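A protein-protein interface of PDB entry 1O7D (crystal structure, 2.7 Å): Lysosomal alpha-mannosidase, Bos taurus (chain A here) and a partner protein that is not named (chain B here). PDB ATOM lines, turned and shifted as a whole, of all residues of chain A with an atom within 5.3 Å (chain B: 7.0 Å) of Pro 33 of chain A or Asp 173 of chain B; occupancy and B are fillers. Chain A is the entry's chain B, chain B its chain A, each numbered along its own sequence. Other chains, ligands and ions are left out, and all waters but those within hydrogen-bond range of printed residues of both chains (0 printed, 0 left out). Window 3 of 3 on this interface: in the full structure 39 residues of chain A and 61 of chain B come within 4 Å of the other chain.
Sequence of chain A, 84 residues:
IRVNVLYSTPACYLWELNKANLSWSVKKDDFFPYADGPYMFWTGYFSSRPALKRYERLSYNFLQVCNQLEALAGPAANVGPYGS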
ATOM      1  N   PHE A  31     -15.518   3.180  11.998  1.00  0.00           N
ATOM      2  CA  PHE A  31     -14.639   3.988  12.829  1.00  0.00           C
ATOM      3  C   PHE A  31     -13.934   3.185  13.942  1.00  0.00           C
ATOM      4  O   PHE A  31     -13.820   3.702  15.040  1.00  0.00           O
ATOM      5  CB  PHE A  31     -15.420   5.105  13.527  1.00  0.00           C
ATOM      6  CG  PHE A  31     -15.886   6.147  12.586  1.00  0.00           C
ATOM      7  CD1 PHE A  31     -15.040   7.178  12.173  1.00  0.00           C
ATOM      8  CD2 PHE A  31     -17.181   6.122  12.124  1.00  0.00           C
ATOM      9  CE1 PHE A  31     -15.511   8.191  11.326  1.00  0.00           C
ATOM     10  CE2 PHE A  31     -17.667   7.119  11.281  1.00  0.00           C
ATOM     11  CZ  PHE A  31     -16.836   8.163  10.881  1.00  0.00           C
ATOM     12  N   PHE A  32     -13.546   1.936  13.733  1.00  0.00           N
ATOM     13  CA  PHE A  32     -12.819   1.142  14.687  1.00  0.00           C
ATOM     14  C   PHE A  32     -11.441   1.110  14.160  1.00  0.00           C
ATOM     15  O   PHE A  32     -11.241   1.052  12.951  1.00  0.00           O
ATOM     16  CB  PHE A  32     -13.419  -0.224  14.736  1.00  0.00           C
ATOM     17  CG  PHE A  32     -14.757  -0.167  15.510  1.00  0.00           C
ATOM     18  CD1 PHE A  32     -14.806   0.075  16.921  1.00  0.00           C
ATOM     19  CD2 PHE A  32     -15.966  -0.326  14.844  1.00  0.00           C
ATOM     20  CE1 PHE A  32     -16.083   0.145  17.598  1.00  0.00           C
ATOM     21  CE2 PHE A  32     -17.188  -0.257  15.493  1.00  0.00           C
ATOM     22  CZ  PHE A  32     -17.242  -0.049  16.853  1.00  0.00           C
ATOM     23  N   PRO A  33     -10.422   1.108  15.041  1.00  0.00           N
ATOM     24  CA  PRO A  33     -10.482   1.146  16.513  1.00  0.00           C
ATOM     25  C   PRO A  33     -10.519   2.560  17.021  1.00  0.00           C
ATOM     26  O   PRO A  33      -9.940   3.474  16.424  1.00  0.00           O
ATOM     27  CB  PRO A  33      -9.195   0.421  16.929  1.00  0.00           C
ATOM     28  CG  PRO A  33      -8.845  -0.384  15.756  1.00  0.00           C
ATOM     29  CD  PRO A  33      -9.152   0.492  14.588  1.00  0.00           C
ATOM     30  N   TYR A  34     -11.212   2.740  18.129  1.00  0.00           N
ATOM     31  CA  TYR A  34     -11.275   4.035  18.777  1.00  0.00           C
ATOM     32  C   TYR A  34     -10.051   4.208  19.697  1.00  0.00           C
ATOM     33  O   TYR A  34      -9.694   3.300  20.434  1.00  0.00           O
ATOM     34  CB  TYR A  34     -12.533   4.117  19.617  1.00  0.00           C
ATOM     35  CG  TYR A  34     -12.542   5.398  20.426  1.00  0.00           C
ATOM     36  CD1 TYR A  34     -12.272   6.667  19.861  1.00  0.00           C
ATOM     37  CD2 TYR A  34     -12.805   5.339  21.773  1.00  0.00           C
ATOM     38  CE1 TYR A  34     -12.289   7.842  20.679  1.00  0.00           C
ATOM     39  CE2 TYR A  34     -12.831   6.470  22.572  1.00  0.00           C
ATOM     40  CZ  TYR A  34     -12.559   7.723  22.004  1.00  0.00           C
ATOM     41  OH  TYR A  34     -12.538   8.872  22.731  1.00  0.00           O
ATOM     42  N   ALA A  35      -9.400   5.363  19.655  1.00  0.00           N
ATOM     43  CA  ALA A  35      -8.240   5.633  20.511  1.00  0.00           C
ATOM     44  C   ALA A  35      -8.161   7.124  20.844  1.00  0.00           C
ATOM     45  O   ALA A  35      -7.920   7.965  19.963  1.00  0.00           O
ATOM     46  CB  ALA A  35      -6.983   5.197  19.822  1.00  0.00           C
ATOM     47  N   PHE A  41      -6.088   2.193  23.629  1.00  0.00           N
ATOM     48  CA  PHE A  41      -7.175   1.861  22.729  1.00  0.00           C
ATOM     49  C   PHE A  41      -8.368   1.338  23.484  1.00  0.00           C
ATOM     50  O   PHE A  41      -8.226   0.633  24.488  1.00  0.00           O
ATOM     51  CB  PHE A  41      -6.731   0.802  21.736  1.00  0.00           C
ATOM     52  CG  PHE A  41      -5.795   1.320  20.694  1.00  0.00           C
ATOM     53  CD1 PHE A  41      -6.282   1.911  19.525  1.00  0.00           C
ATOM     54  CD2 PHE A  41      -4.418   1.225  20.879  1.00  0.00           C
ATOM     55  CE1 PHE A  41      -5.409   2.404  18.554  1.00  0.00           C
ATOM     56  CE2 PHE A  41      -3.532   1.715  19.915  1.00  0.00           C
ATOM     57  CZ  PHE A  41      -4.032   2.305  18.747  1.00  0.00           C
ATOM     58  N   THR A  43     -10.259  -1.030  22.902  1.00  0.00           N
ATOM     59  CA  THR A  43     -10.570  -2.300  22.276  1.00  0.00           C
ATOM     60  C   THR A  43     -10.711  -3.454  23.270  1.00  0.00           C
ATOM     61  O   THR A  43     -10.935  -4.598  22.880  1.00  0.00           O
ATOM     62  CB  THR A  43      -9.504  -2.659  21.227  1.00  0.00           C
ATOM     63  OG1 THR A  43      -8.227  -2.791  21.862  1.00  0.00           O
ATOM     64  CG2 THR A  43      -9.434  -1.565  20.166  1.00  0.00           C
ATOM     65  N   PHE B 149     -17.910   4.237  21.958  1.00  0.00           N
ATOM     66  CA  PHE B 149     -16.471   4.164  21.688  1.00  0.00           C
ATOM     67  C   PHE B 149     -16.095   3.658  20.280  1.00  0.00           C
ATOM     68  O   PHE B 149     -15.543   2.558  20.110  1.00  0.00           O
ATOM     69  CB  PHE B 149     -15.831   3.276  22.762  1.00  0.00           C
ATOM     70  CG  PHE B 149     -16.591   3.256  24.070  1.00  0.00           C
ATOM     71  CD1 PHE B 149     -16.796   2.053  24.749  1.00  0.00           C
ATOM     72  CD2 PHE B 149     -17.131   4.419  24.604  1.00  0.00           C
ATOM     73  CE1 PHE B 149     -17.528   2.006  25.940  1.00  0.00           C
ATOM     74  CE2 PHE B 149     -17.867   4.385  25.796  1.00  0.00           C
ATOM     75  CZ  PHE B 149     -18.069   3.174  26.463  1.00  0.00           C
ATOM     76  N   GLY B 150     -16.364   4.482  19.273  1.00  0.00           N
ATOM     77  CA  GLY B 150     -16.078   4.072  17.911  1.00  0.00           C
ATOM     78  C   GLY B 150     -17.416   3.811  17.262  1.00  0.00           C
ATOM     79  O   GLY B 150     -18.411   3.664  17.962  1.00  0.00           O
ATOM     80  N   GLY B 170     -19.350  12.112  19.020  1.00  0.00           N
ATOM     81  CA  GLY B 170     -18.173  12.670  19.666  1.00  0.00           C
ATOM     82  C   GLY B 170     -16.884  11.869  19.599  1.00  0.00           C
ATOM     83  O   GLY B 170     -15.841  12.417  19.270  1.00  0.00           O
ATOM     84  N   ARG B 171     -16.927  10.577  19.881  1.00  0.00           N
ATOM     85  CA  ARG B 171     -15.692   9.806  19.875  1.00  0.00           C
ATOM     86  C   ARG B 171     -15.177   9.206  18.561  1.00  0.00           C
ATOM     87  O   ARG B 171     -15.851   8.366  17.950  1.00  0.00           O
ATOM     88  CB  ARG B 171     -15.788   8.687  20.904  1.00  0.00           C
ATOM     89  CG  ARG B 171     -16.086   9.180  22.292  1.00  0.00           C
ATOM     90  CD  ARG B 171     -16.300   8.032  23.261  1.00  0.00           C
ATOM     91  NE  ARG B 171     -16.621   8.551  24.580  1.00  0.00           N
ATOM     92  CZ  ARG B 171     -15.732   9.132  25.372  1.00  0.00           C
ATOM     93  NH1 ARG B 171     -14.480   9.243  24.960  1.00  0.00           N
ATOM     94  NH2 ARG B 171     -16.095   9.613  26.556  1.00  0.00           N
ATOM     95  N   LEU B 172     -13.984   9.639  18.145  1.00  0.00           N
ATOM     96  CA  LEU B 172     -13.325   9.105  16.960  1.00  0.00           C
ATOM     97  C   LEU B 172     -11.848   9.117  17.267  1.00  0.00           C
ATOM     98  O   LEU B 172     -11.399   9.858  18.134  1.00  0.00           O
ATOM     99  CB  LEU B 172     -13.598   9.931  15.696  1.00  0.00           C
ATOM    100  CG  LEU B 172     -12.929  11.276  15.428  1.00  0.00           C
ATOM    101  CD1 LEU B 172     -13.193  11.692  13.996  1.00  0.00           C
ATOM    102  CD2 LEU B 172     -13.459  12.307  16.405  1.00  0.00           C
ATOM    103  N   ASP B 173     -11.095   8.286  16.561  1.00  0.00           N
ATOM    104  CA  ASP B 173      -9.662   8.189  16.784  1.00  0.00           C
ATOM    105  C   ASP B 173      -9.031   9.574  16.831  1.00  0.00           C
ATOM    106  O   ASP B 173      -9.387  10.454  16.039  1.00  0.00           O
ATOM    107  CB  ASP B 173      -9.010   7.374  15.680  1.00  0.00           C
ATOM    108  CG  ASP B 173      -7.649   6.874  16.081  1.00  0.00           C
ATOM    109  OD1 ASP B 173      -6.828   7.718  16.504  1.00  0.00           O
ATOM    110  OD2 ASP B 173      -7.397   5.645  15.989  1.00  0.00           O
ATOM    111  N   TYR B 174      -8.088   9.779  17.745  1.00  0.00           N
ATOM    112  CA  TYR B 174      -7.475  11.096  17.840  1.00  0.00           C
ATOM    113  C   TYR B 174      -6.729  11.494  16.566  1.00  0.00           C
ATOM    114  O   TYR B 174      -6.799  12.652  16.162  1.00  0.00           O
ATOM    115  CB  TYR B 174      -6.556  11.207  19.069  1.00  0.00           C
ATOM    116  CG  TYR B 174      -5.301  10.387  18.994  1.00  0.00           C
ATOM    117  CD1 TYR B 174      -5.341   8.996  19.101  1.00  0.00           C
ATOM    118  CD2 TYR B 174      -4.074  10.994  18.770  1.00  0.00           C
ATOM    119  CE1 TYR B 174      -4.182   8.226  18.977  1.00  0.00           C
ATOM    120  CE2 TYR B 174      -2.912  10.241  18.645  1.00  0.00           C
ATOM    121  CZ  TYR B 174      -2.969   8.856  18.746  1.00  0.00           C
ATOM    122  OH  TYR B 174      -1.814   8.108  18.591  1.00  0.00           O
ATOM    123  N   GLN B 175      -6.042  10.552  15.921  1.00  0.00           N
ATOM    124  CA  GLN B 175      -5.314  10.885  14.698  1.00  0.00           C
ATOM    125  C   GLN B 175      -6.293  11.221  13.587  1.00  0.00           C
ATOM    126  O   GLN B 175      -6.018  12.102  12.773  1.00  0.00           O
ATOM    127  CB  GLN B 175      -4.417   9.735  14.223  1.00  0.00           C
ATOM    128  CG  GLN B 175      -3.428   9.220  15.241  1.00  0.00           C
ATOM    129  CD  GLN B 175      -2.364   8.339  14.611  1.00  0.00           C
ATOM    130  OE1 GLN B 175      -2.574   7.740  13.554  1.00  0.00           O
ATOM    131  NE2 GLN B 175      -1.216   8.245  15.265  1.00  0.00           N
ATOM    132  N   ASP B 176      -7.425  10.518  13.553  1.00  0.00           N
ATOM    133  CA  ASP B 176      -8.432  10.766  12.528  1.00  0.00           C
ATOM    134  C   ASP B 176      -8.964  12.180  12.685  1.00  0.00           C
ATOM    135  O   ASP B 176      -9.085  12.910  11.715  1.00  0.00           O
ATOM    136  CB  ASP B 176      -9.587   9.754  12.637  1.00  0.00           C
ATOM    137  CG  ASP B 176     -10.504   9.752  11.395  1.00  0.00           C
ATOM    138  OD1 ASP B 176     -10.021  10.129  10.300  1.00  0.00           O
ATOM    139  OD2 ASP B 176     -11.693   9.361  11.507  1.00  0.00           O
ATOM    140  N   LYS B 177      -9.264  12.565  13.919  1.00  0.00           N
ATOM    141  CA  LYS B 177      -9.783  13.895  14.188  1.00  0.00           C
ATOM    142  C   LYS B 177      -8.811  14.969  13.740  1.00  0.00           C
ATOM    143  O   LYS B 177      -9.191  15.885  13.010  1.00  0.00           O
ATOM    144  CB  LYS B 177     -10.065  14.066  15.678  1.00  0.00           C
ATOM    145  CG  LYS B 177     -10.854  15.326  16.006  1.00  0.00           C
ATOM    146  CD  LYS B 177     -11.272  15.356  17.460  1.00  0.00           C
ATOM    147  CE  LYS B 177     -12.230  16.493  17.759  1.00  0.00           C
ATOM    148  NZ  LYS B 177     -12.677  16.497  19.189  1.00  0.00           N
ATOM    149  N   LYS B 178      -7.561  14.858  14.181  1.00  0.00           N
ATOM    150  CA  LYS B 178      -6.528  15.823  13.832  1.00  0.00           C
ATOM    151  C   LYS B 178      -6.545  16.088  12.337  1.00  0.00           C
ATOM    152  O   LYS B 178      -6.644  17.234  11.901  1.00  0.00           O
ATOM    153  CB  LYS B 178      -5.148  15.298  14.230  1.00  0.00           C
ATOM    154  CG  LYS B 178      -3.995  16.189  13.756  1.00  0.00           C
ATOM    155  CD  LYS B 178      -2.641  15.436  13.629  1.00  0.00           C
ATOM    156  CE  LYS B 178      -2.449  14.717  12.261  1.00  0.00           C
ATOM    157  NZ  LYS B 178      -2.917  13.290  12.175  1.00  0.00           N
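Among the printed residues, pairs that only touch across the chains: Phe 31 of chain A with Gly 150 of chain B (3.7 Å), Phe 31 of chain A with Asp 176 of chain B (3.997 Å), Phe 32 of chain A with Phe 149 of chain B (3.5 Å), Phe 32 of chain A with Gly 150 of chain B (3.9 Å), Tyr 34 of chain A with Phe 149 of chain B (3.4 Å), Tyr 34 of chain A with Gly 150 of chain B (3.9 Å), Tyr 34 of chain A with Leu 172 of chain B (3.4 Å), Tyr 34 of chain A with Asp 173 of chain B (3.9 Å) and Ala 35 of chain A with Asp 173 of chain B (3.6 Å).
The side-chain hydroxyl of Tyr 34 of chain A sits at hydrogen-bond distance from the guanidinium group of Arg 171 of chain B, 3.0 Å away. The backbone carbonyl oxygen of Pro 33 of chain A lies close to the side-chain carboxylate of Asp 173 of chain B (3.4 Å). The backbone carbonyl oxygen of Ala 35 of chain A is in hydrogen-bond range of the backbone NH of Tyr 174 of chain B (2.9 Å).
OH of Tyr 174 of chain B lies within hydrogen-bond range of NE2 of Gln 175 of chain B (3.4 Å). The backbone NH (N) of Gln 175 of chain B is in hydrogen-bond range of the side-chain carboxylate (OD1) of Asp 173 of chain B (3.0 Å).
Printed residues of chain B within 4 Å of Phe 31 of chain A: Gly 150 and Asp 176. Pro 33 of chain A touches just one residue of chain B: Asp 173 (3.4 Å). Asp 173 of chain B touches just these residues of chain A: Pro 33, Tyr 34 and Ala 35. Gln 175 of chain B touches none of the printed residues of chain A. Of the printed residues of chain A, Asp 176 of chain B touches Phe 31. Lys 178 of chain B touches none of the printed residues of chain A. The nearest residue of chain A that does not touch Asp 173 of chain B is Phe 41 of chain A (4.6 Å). The nearest printed residue of chain B that does not touch Ala 35 of chain A is Leu 172 of chain B (4.4 Å).
Hydrophobic or aromatic side chains of chain B within 4 Å of the printed part of chain A: Phe 149 and Tyr 174. Along chain B the printed residues that touch a printed residue of chain A span positions 149 to 176. Of the 7 printed residues of chain A, 5 touch a printed residue of chain B. Hydrophobic or aromatic side chains of chain A within 4 Å of the printed part of chain B: Phe 31, Phe 32, Tyr 34 and Ala 35.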
